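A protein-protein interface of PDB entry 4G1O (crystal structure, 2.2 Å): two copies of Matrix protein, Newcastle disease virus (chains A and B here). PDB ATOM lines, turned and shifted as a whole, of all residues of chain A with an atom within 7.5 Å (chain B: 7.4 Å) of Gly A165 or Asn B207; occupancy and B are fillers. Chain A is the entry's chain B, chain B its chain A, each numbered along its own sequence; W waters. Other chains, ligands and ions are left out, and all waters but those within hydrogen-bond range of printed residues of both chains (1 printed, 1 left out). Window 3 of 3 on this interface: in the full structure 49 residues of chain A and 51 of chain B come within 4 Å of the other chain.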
ATOM      1  N   GLN A  67      28.510  -9.525   5.641  1.00  0.00           N
ATOM      2  CA  GLN A  67      28.361 -10.948   5.572  1.00  0.00           C
ATOM      3  C   GLN A  67      27.765 -11.385   6.926  1.00  0.00           C
ATOM      4  O   GLN A  67      28.412 -11.294   7.981  1.00  0.00           O
ATOM      5  CB  GLN A  67      29.745 -11.557   5.338  1.00  0.00           C
ATOM      6  CG  GLN A  67      29.869 -13.010   5.725  1.00  0.00           C
ATOM      7  CD  GLN A  67      29.456 -13.902   4.611  1.00  0.00           C
ATOM      8  OE1 GLN A  67      30.247 -14.192   3.721  1.00  0.00           O
ATOM      9  NE2 GLN A  67      28.197 -14.332   4.633  1.00  0.00           N
ATOM     10  N   LYS A 118      22.731 -10.225  -3.092  1.00  0.00           N
ATOM     11  CA  LYS A 118      23.563 -11.341  -3.577  1.00  0.00           C
ATOM     12  C   LYS A 118      24.130 -10.978  -4.956  1.00  0.00           C
ATOM     13  O   LYS A 118      23.566 -10.152  -5.669  1.00  0.00           O
ATOM     14  CB  LYS A 118      22.685 -12.563  -3.699  1.00  0.00           C
ATOM     15  CG  LYS A 118      21.523 -12.221  -4.667  1.00  0.00           C
ATOM     16  CD  LYS A 118      20.407 -13.254  -4.600  1.00  0.00           C
ATOM     17  CE  LYS A 118      20.860 -14.652  -5.013  1.00  0.00           C
ATOM     18  NZ  LYS A 118      19.643 -15.488  -5.307  1.00  0.00           N
ATOM     19  N   LYS A 119      25.248 -11.574  -5.329  1.00  0.00           N
ATOM     20  CA  LYS A 119      25.760 -11.451  -6.712  1.00  0.00           C
ATOM     21  C   LYS A 119      24.849 -12.184  -7.711  1.00  0.00           C
ATOM     22  O   LYS A 119      24.269 -13.238  -7.403  1.00  0.00           O
ATOM     23  CB  LYS A 119      27.174 -12.046  -6.796  1.00  0.00           C
ATOM     24  CG  LYS A 119      28.201 -11.235  -6.047  1.00  0.00           C
ATOM     25  CD  LYS A 119      28.826 -10.167  -6.944  1.00  0.00           C
ATOM     26  CE  LYS A 119      30.149 -10.662  -7.498  1.00  0.00           C
ATOM     27  NZ  LYS A 119      31.432 -10.085  -6.968  1.00  0.00           N
ATOM     28  N   SER A 120      24.681 -11.611  -8.883  1.00  0.00           N
ATOM     29  CA  SER A 120      24.173 -12.330 -10.061  1.00  0.00           C
ATOM     30  C   SER A 120      25.054 -11.801 -11.237  1.00  0.00           C
ATOM     31  O   SER A 120      26.060 -11.146 -10.969  1.00  0.00           O
ATOM     32  CB  SER A 120      22.689 -12.106 -10.258  1.00  0.00           C
ATOM     33  OG  SER A 120      22.132 -12.994 -11.230  1.00  0.00           O
ATOM     34  N   PRO A 160      33.483  -5.047  -5.504  1.00  0.00           N
ATOM     35  CA  PRO A 160      32.729  -6.294  -5.779  1.00  0.00           C
ATOM     36  C   PRO A 160      33.564  -7.579  -5.674  1.00  0.00           C
ATOM     37  O   PRO A 160      33.019  -8.686  -5.477  1.00  0.00           O
ATOM     38  CB  PRO A 160      32.273  -6.110  -7.234  1.00  0.00           C
ATOM     39  CG  PRO A 160      33.172  -5.062  -7.795  1.00  0.00           C
ATOM     40  CD  PRO A 160      33.459  -4.121  -6.649  1.00  0.00           C
ATOM     41  N   LYS A 162      35.407  -8.360  -3.376  1.00  0.00           N
ATOM     42  CA  LYS A 162      35.433  -8.781  -1.961  1.00  0.00           C
ATOM     43  C   LYS A 162      34.041  -9.305  -1.559  1.00  0.00           C
ATOM     44  O   LYS A 162      33.782  -9.675  -0.417  1.00  0.00           O
ATOM     45  CB  LYS A 162      35.798  -7.567  -1.102  1.00  0.00           C
ATOM     46  CG  LYS A 162      36.556  -7.809   0.206  1.00  0.00           C
ATOM     47  CD  LYS A 162      36.670  -6.443   0.855  1.00  0.00           C
ATOM     48  CE  LYS A 162      36.982  -6.495   2.338  1.00  0.00           C
ATOM     49  NZ  LYS A 162      38.392  -6.911   2.540  1.00  0.00           N
ATOM     50  N   ILE A 163      33.105  -9.283  -2.490  1.00  0.00           N
ATOM     51  CA  ILE A 163      31.762  -9.787  -2.187  1.00  0.00           C
ATOM     52  C   ILE A 163      31.773 -11.281  -2.545  1.00  0.00           C
ATOM     53  O   ILE A 163      32.172 -11.607  -3.649  1.00  0.00           O
ATOM     54  CB  ILE A 163      30.681  -9.033  -3.004  1.00  0.00           C
ATOM     55  CG1 ILE A 163      30.697  -7.525  -2.716  1.00  0.00           C
ATOM     56  CG2 ILE A 163      29.307  -9.631  -2.761  1.00  0.00           C
ATOM     57  CD1 ILE A 163      30.462  -7.117  -1.266  1.00  0.00           C
ATOM     58  N   PRO A 164      31.390 -12.190  -1.608  1.00  0.00           N
ATOM     59  CA  PRO A 164      31.405 -13.619  -1.996  1.00  0.00           C
ATOM     60  C   PRO A 164      30.218 -13.969  -2.899  1.00  0.00           C
ATOM     61  O   PRO A 164      29.202 -13.241  -2.912  1.00  0.00           O
ATOM     62  CB  PRO A 164      31.260 -14.356  -0.661  1.00  0.00           C
ATOM     63  CG  PRO A 164      30.495 -13.384   0.207  1.00  0.00           C
ATOM     64  CD  PRO A 164      30.976 -12.004  -0.201  1.00  0.00           C
ATOM     65  N   GLY A 165      30.340 -15.083  -3.625  1.00  0.00           N
ATOM     66  CA  GLY A 165      29.280 -15.614  -4.473  1.00  0.00           C
ATOM     67  C   GLY A 165      28.130 -16.298  -3.758  1.00  0.00           C
ATOM     68  O   GLY A 165      27.152 -16.652  -4.378  1.00  0.00           O
ATOM     69  N   SER A 166      28.207 -16.484  -2.454  1.00  0.00           N
ATOM     70  CA  SER A 166      27.075 -17.094  -1.738  1.00  0.00           C
ATOM     71  C   SER A 166      27.040 -16.654  -0.272  1.00  0.00           C
ATOM     72  O   SER A 166      27.907 -15.889   0.176  1.00  0.00           O
ATOM     73  CB  SER A 166      27.157 -18.623  -1.817  1.00  0.00           C
ATOM     74  OG  SER A 166      28.264 -19.067  -1.067  1.00  0.00           O
ATOM     75  N   GLY A 167      26.046 -17.131   0.475  1.00  0.00           N
ATOM     76  CA  GLY A 167      25.891 -16.702   1.863  1.00  0.00           C
ATOM     77  C   GLY A 167      24.934 -15.528   1.974  1.00  0.00           C
ATOM     78  O   GLY A 167      24.610 -14.831   0.994  1.00  0.00           O
ATOM     79  N   LEU A 169      23.655 -11.930   2.779  1.00  0.00           N
ATOM     80  CA  LEU A 169      24.285 -10.624   2.844  1.00  0.00           C
ATOM     81  C   LEU A 169      23.285  -9.536   3.142  1.00  0.00           C
ATOM     82  O   LEU A 169      22.295  -9.436   2.434  1.00  0.00           O
ATOM     83  CB  LEU A 169      24.980 -10.290   1.522  1.00  0.00           C
ATOM     84  CG  LEU A 169      26.102 -11.236   1.116  1.00  0.00           C
ATOM     85  CD1 LEU A 169      26.687 -10.810  -0.233  1.00  0.00           C
ATOM     86  CD2 LEU A 169      27.140 -11.177   2.201  1.00  0.00           C
ATOM     87  N   ALA B 205      25.684 -20.085 -14.169  1.00  0.00           N
ATOM     88  CA  ALA B 205      26.721 -19.162 -13.789  1.00  0.00           C
ATOM     89  C   ALA B 205      27.840 -19.885 -13.089  1.00  0.00           C
ATOM     90  O   ALA B 205      27.671 -21.013 -12.657  1.00  0.00           O
ATOM     91  CB  ALA B 205      26.137 -18.087 -12.887  1.00  0.00           C
ATOM     92  N   LEU B 206      28.977 -19.220 -12.982  1.00  0.00           N
ATOM     93  CA  LEU B 206      30.132 -19.723 -12.268  1.00  0.00           C
ATOM     94  C   LEU B 206      30.540 -18.791 -11.107  1.00  0.00           C
ATOM     95  O   LEU B 206      30.846 -17.609 -11.316  1.00  0.00           O
ATOM     96  CB  LEU B 206      31.307 -19.874 -13.241  1.00  0.00           C
ATOM     97  CG  LEU B 206      31.208 -20.838 -14.420  1.00  0.00           C
ATOM     98  CD1 LEU B 206      32.486 -20.685 -15.230  1.00  0.00           C
ATOM     99  CD2 LEU B 206      31.041 -22.285 -13.996  1.00  0.00           C
ATOM    100  N   ASN B 207      30.539 -19.342  -9.893  1.00  0.00           N
ATOM    101  CA  ASN B 207      31.097 -18.721  -8.707  1.00  0.00           C
ATOM    102  C   ASN B 207      32.603 -18.962  -8.777  1.00  0.00           C
ATOM    103  O   ASN B 207      33.068 -20.033  -8.427  1.00  0.00           O
ATOM    104  CB  ASN B 207      30.487 -19.380  -7.426  1.00  0.00           C
ATOM    105  CG  ASN B 207      30.991 -18.748  -6.109  1.00  0.00           C
ATOM    106  OD1 ASN B 207      31.930 -17.942  -6.096  1.00  0.00           O
ATOM    107  ND2 ASN B 207      30.353 -19.107  -4.994  1.00  0.00           N
ATOM    108  N   VAL B 208      33.358 -17.975  -9.243  1.00  0.00           N
ATOM    109  CA  VAL B 208      34.780 -18.160  -9.466  1.00  0.00           C
ATOM    110  C   VAL B 208      35.540 -17.449  -8.350  1.00  0.00           C
ATOM    111  O   VAL B 208      35.222 -16.309  -8.003  1.00  0.00           O
ATOM    112  CB  VAL B 208      35.191 -17.550 -10.820  1.00  0.00           C
ATOM    113  CG1 VAL B 208      36.720 -17.537 -10.981  1.00  0.00           C
ATOM    114  CG2 VAL B 208      34.494 -18.271 -11.980  1.00  0.00           C
ATOM    115  N   THR B 209      36.528 -18.108  -7.753  1.00  0.00           N
ATOM    116  CA  THR B 209      37.410 -17.384  -6.812  1.00  0.00           C
ATOM    117  C   THR B 209      38.826 -17.452  -7.348  1.00  0.00           C
ATOM    118  O   THR B 209      39.208 -18.457  -7.930  1.00  0.00           O
ATOM    119  CB  THR B 209      37.342 -17.895  -5.358  1.00  0.00           C
ATOM    120  OG1 THR B 209      37.789 -19.240  -5.320  1.00  0.00           O
ATOM    121  CG2 THR B 209      35.916 -17.835  -4.793  1.00  0.00           C
ATOM    122  N   ALA B 233      40.371 -13.002  -4.929  1.00  0.00           N
ATOM    123  CA  ALA B 233      39.278 -12.179  -5.475  1.00  0.00           C
ATOM    124  C   ALA B 233      38.050 -12.991  -5.945  1.00  0.00           C
ATOM    125  O   ALA B 233      38.150 -14.153  -6.340  1.00  0.00           O
ATOM    126  CB  ALA B 233      39.789 -11.306  -6.613  1.00  0.00           C
ATOM    127  N   ASN B 234      36.885 -12.362  -5.898  1.00  0.00           N
ATOM    128  CA  ASN B 234      35.655 -13.047  -6.250  1.00  0.00           C
ATOM    129  C   ASN B 234      35.025 -12.491  -7.500  1.00  0.00           C
ATOM    130  O   ASN B 234      35.004 -11.280  -7.701  1.00  0.00           O
ATOM    131  CB  ASN B 234      34.643 -12.965  -5.128  1.00  0.00           C
ATOM    132  CG  ASN B 234      35.203 -13.457  -3.826  1.00  0.00           C
ATOM    133  OD1 ASN B 234      35.036 -14.639  -3.479  1.00  0.00           O
ATOM    134  ND2 ASN B 234      35.929 -12.568  -3.106  1.00  0.00           N
ATOM    135  N   LEU B 235      34.457 -13.403  -8.283  1.00  0.00           N
ATOM    136  CA  LEU B 235      33.932 -13.096  -9.596  1.00  0.00           C
ATOM    137  C   LEU B 235      32.796 -14.052  -9.854  1.00  0.00           C
ATOM    138  O   LEU B 235      32.962 -15.261  -9.641  1.00  0.00           O
ATOM    139  CB  LEU B 235      35.024 -13.250 -10.657  1.00  0.00           C
ATOM    140  CG  LEU B 235      34.527 -13.297 -12.093  1.00  0.00           C
ATOM    141  CD1 LEU B 235      33.727 -12.061 -12.588  1.00  0.00           C
ATOM    142  CD2 LEU B 235      35.752 -13.527 -12.952  1.00  0.00           C
ATOM    143  N   PHE B 236      31.649 -13.495 -10.262  1.00  0.00           N
ATOM    144  CA  PHE B 236      30.448 -14.257 -10.520  1.00  0.00           C
ATOM    145  C   PHE B 236      30.126 -14.096 -11.991  1.00  0.00           C
ATOM    146  O   PHE B 236      29.892 -12.996 -12.465  1.00  0.00           O
ATOM    147  CB  PHE B 236      29.296 -13.725  -9.691  1.00  0.00           C
ATOM    148  CG  PHE B 236      28.168 -14.715  -9.515  1.00  0.00           C
ATOM    149  CD1 PHE B 236      27.098 -14.768 -10.424  1.00  0.00           C
ATOM    150  CD2 PHE B 236      28.168 -15.586  -8.424  1.00  0.00           C
ATOM    151  CE1 PHE B 236      26.045 -15.656 -10.220  1.00  0.00           C
ATOM    152  CE2 PHE B 236      27.139 -16.498  -8.241  1.00  0.00           C
ATOM    153  CZ  PHE B 236      26.070 -16.537  -9.141  1.00  0.00           C
ATOM    154  N   LEU B 237      30.104 -15.189 -12.729  1.00  0.00           N
ATOM    155  CA  LEU B 237      30.203 -15.051 -14.181  1.00  0.00           C
ATOM    156  C   LEU B 237      29.064 -15.788 -14.840  1.00  0.00           C
ATOM    157  O   LEU B 237      28.920 -17.004 -14.642  1.00  0.00           O
ATOM    158  CB  LEU B 237      31.570 -15.622 -14.626  1.00  0.00           C
ATOM    159  CG  LEU B 237      31.955 -15.458 -16.099  1.00  0.00           C
ATOM    160  CD1 LEU B 237      32.106 -13.972 -16.443  1.00  0.00           C
ATOM    161  CD2 LEU B 237      33.226 -16.238 -16.427  1.00  0.00           C
ATOM    162  N   SER B 324      38.947 -21.666  -6.987  1.00  0.00           N
ATOM    163  CA  SER B 324      37.829 -22.602  -7.126  1.00  0.00           C
ATOM    164  C   SER B 324      36.815 -22.032  -8.099  1.00  0.00           C
ATOM    165  O   SER B 324      36.656 -20.810  -8.220  1.00  0.00           O
ATOM    166  CB  SER B 324      37.159 -22.907  -5.783  1.00  0.00           C
ATOM    167  OG  SER B 324      36.650 -21.716  -5.208  1.00  0.00           O
ATOM    168  N   VAL B 325      36.149 -22.929  -8.802  1.00  0.00           N
ATOM    169  CA  VAL B 325      35.126 -22.543  -9.760  1.00  0.00           C
ATOM    170  C   VAL B 325      33.928 -23.411  -9.453  1.00  0.00           C
ATOM    171  O   VAL B 325      34.041 -24.632  -9.557  1.00  0.00           O
ATOM    172  CB  VAL B 325      35.595 -22.861 -11.191  1.00  0.00           C
ATOM    173  CG1 VAL B 325      34.549 -22.443 -12.220  1.00  0.00           C
ATOM    174  CG2 VAL B 325      36.942 -22.193 -11.467  1.00  0.00           C
ATOM    175  N   LYS B 326      32.798 -22.816  -9.057  1.00  0.00           N
ATOM    176  CA  LYS B 326      31.587 -23.612  -8.798  1.00  0.00           C
ATOM    177  C   LYS B 326      30.451 -23.241  -9.768  1.00  0.00           C
ATOM    178  O   LYS B 326      30.222 -22.053 -10.062  1.00  0.00           O
ATOM    179  CB  LYS B 326      31.109 -23.475  -7.335  1.00  0.00           C
ATOM    180  CG  LYS B 326      32.145 -22.949  -6.323  1.00  0.00           C
ATOM    181  CD  LYS B 326      32.597 -23.967  -5.297  1.00  0.00           C
ATOM    182  CE  LYS B 326      33.449 -25.055  -5.936  1.00  0.00           C
ATOM    183  NZ  LYS B 326      33.914 -26.091  -4.961  1.00  0.00           N
ATOM    184  N   VAL B 327      29.743 -24.265 -10.240  1.00  0.00           N
ATOM    185  CA  VAL B 327      28.647 -24.111 -11.206  1.00  0.00           C
ATOM    186  C   VAL B 327      27.331 -23.964 -10.474  1.00  0.00           C
ATOM    187  O   VAL B 327      26.905 -24.884  -9.790  1.00  0.00           O
ATOM    188  CB  VAL B 327      28.544 -25.316 -12.167  1.00  0.00           C
ATOM    189  CG1 VAL B 327      27.455 -25.089 -13.194  1.00  0.00           C
ATOM    190  CG2 VAL B 327      29.840 -25.548 -12.905  1.00  0.00           C
ATOM    191  N   ILE B 328      26.702 -22.803 -10.659  1.00  0.00           N
ATOM    192  CA  ILE B 328      25.533 -22.353  -9.912  1.00  0.00           C
ATOM    193  C   ILE B 328      24.368 -22.195 -10.877  1.00  0.00           C
ATOM    194  O   ILE B 328      24.542 -21.583 -11.940  1.00  0.00           O
ATOM    195  CB  ILE B 328      25.846 -20.967  -9.295  1.00  0.00           C
ATOM    196  CG1 ILE B 328      27.088 -21.053  -8.393  1.00  0.00           C
ATOM    197  CG2 ILE B 328      24.669 -20.389  -8.505  1.00  0.00           C
ATOM    198  CD1 ILE B 328      26.965 -22.062  -7.278  1.00  0.00           C
ATOM    199  N   GLN B 330      20.965 -20.226 -11.182  1.00  0.00           N
ATOM    200  CA  GLN B 330      20.181 -19.144 -10.600  1.00  0.00           C
ATOM    201  C   GLN B 330      18.906 -19.122 -11.430  1.00  0.00           C
ATOM    202  O   GLN B 330      18.875 -19.664 -12.568  1.00  0.00           O
ATOM    203  CB  GLN B 330      20.887 -17.783 -10.706  1.00  0.00           C
ATOM    204  CG  GLN B 330      22.057 -17.540  -9.742  1.00  0.00           C
ATOM    205  CD  GLN B 330      22.555 -16.086  -9.696  1.00  0.00           C
ATOM    206  OE1 GLN B 330      22.724 -15.474 -10.730  1.00  0.00           O
ATOM    207  NE2 GLN B 330      22.859 -15.559  -8.476  1.00  0.00           N
ATOM    208  N   ASP B 342      20.013 -19.658  -4.726  1.00  0.00           N
ATOM    209  CA  ASP B 342      20.932 -20.262  -5.709  1.00  0.00           C
ATOM    210  C   ASP B 342      21.096 -21.736  -5.437  1.00  0.00           C
ATOM    211  O   ASP B 342      20.970 -22.200  -4.293  1.00  0.00           O
ATOM    212  CB  ASP B 342      22.313 -19.588  -5.703  1.00  0.00           C
ATOM    213  CG  ASP B 342      22.244 -18.144  -6.174  1.00  0.00           C
ATOM    214  OD1 ASP B 342      21.146 -17.699  -6.630  1.00  0.00           O
ATOM    215  OD2 ASP B 342      23.285 -17.441  -6.070  1.00  0.00           O
ATOM    216  N   GLU B 344      23.937 -24.573  -6.009  1.00  0.00           N
ATOM    217  CA  GLU B 344      25.282 -25.026  -6.434  1.00  0.00           C
ATOM    218  C   GLU B 344      25.207 -26.444  -7.046  1.00  0.00           C
ATOM    219  O   GLU B 344      24.736 -27.372  -6.403  1.00  0.00           O
ATOM    220  CB  GLU B 344      26.303 -24.971  -5.262  1.00  0.00           C
ATOM    221  CG  GLU B 344      27.724 -25.462  -5.591  1.00  0.00           C
ATOM    222  CD  GLU B 344      28.713 -25.377  -4.410  1.00  0.00           C
ATOM    223  OE1 GLU B 344      28.607 -24.461  -3.573  1.00  0.00           O
ATOM    224  OE2 GLU B 344      29.635 -26.218  -4.313  1.00  0.00           O
HETATM  225  O   HOH W   1      34.056  -8.854  -8.727  1.00  0.00           O
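Lys A119 touches Asn B234. Phe B236 touches Lys A119. Phe B236 touches Ser A120 (CD1 to C, 3.7 Å). O of Pro A160 touches O of Asn B234 (3.95 Å). Lys A162 touches Asn B234. CB of Asn B234 touches O of Ile A163, at 3.2 Å. Asn B207 touches Gly A165 (ND2 to CA, 3.7 Å). Gly A165 touches Phe B236 (O to CE2, 3.9 Å).
No position is printed for both chains. Of the 11 pairs that touch across the chains among the printed residues, none has its exchanged pair printed and touching as well.
Of the 18 printed residues of chain B, 5 touch a printed residue of chain A. Among the printed residues, 11 pairs touch across the chains.
NE2 of Gln B330 is in hydrogen-bond range of O of Lys A119 (2.9 Å). OE1 of Gln B330 lies within hydrogen-bond range of OG of Ser A120 (2.6 Å). OD1 of Asp B342 lies within salt-bridge range of NZ of Lys A118, at 3.0 Å.
Water W1 lies within hydrogen-bond range of O of Asn B234 (2.8 Å), NZ of Lys A119 (3.4 Å) and O of Pro A160 (3.4 Å).
N of Asn B207 is in hydrogen-bond range of O of Lys B326 (2.7 Å). NE2 of Gln B330 is in hydrogen-bond range of OD2 of Asp B342 (3.1 Å). O of Pro A160 is in hydrogen-bond range of NZ of Lys A119 (2.6 Å).
Gly A165 touches two residues of chain B. Of the printed residues of chain A, Gln B330 touches Lys A119 and Ser A120. Of the printed residues of chain B, Lys A118 touches Asp B342. Of the printed residues of chain B, Ser A120 touches Phe B236 and Gln B330. Printed residues of chain A within 4 Å of Phe B236: Lys A119, Ser A120 and Gly A165. Of the printed residues of chain B, Lys A162 touches Asn B234 (3.99 Å). Ala B233 touches none of the printed residues of chain A. The nearest residue of chain A that does not touch Asn B207 is Ser A166 (4.2 Å). The nearest printed residue of chain B that does not touch Lys A118 is Gln B330 (4.1 Å).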
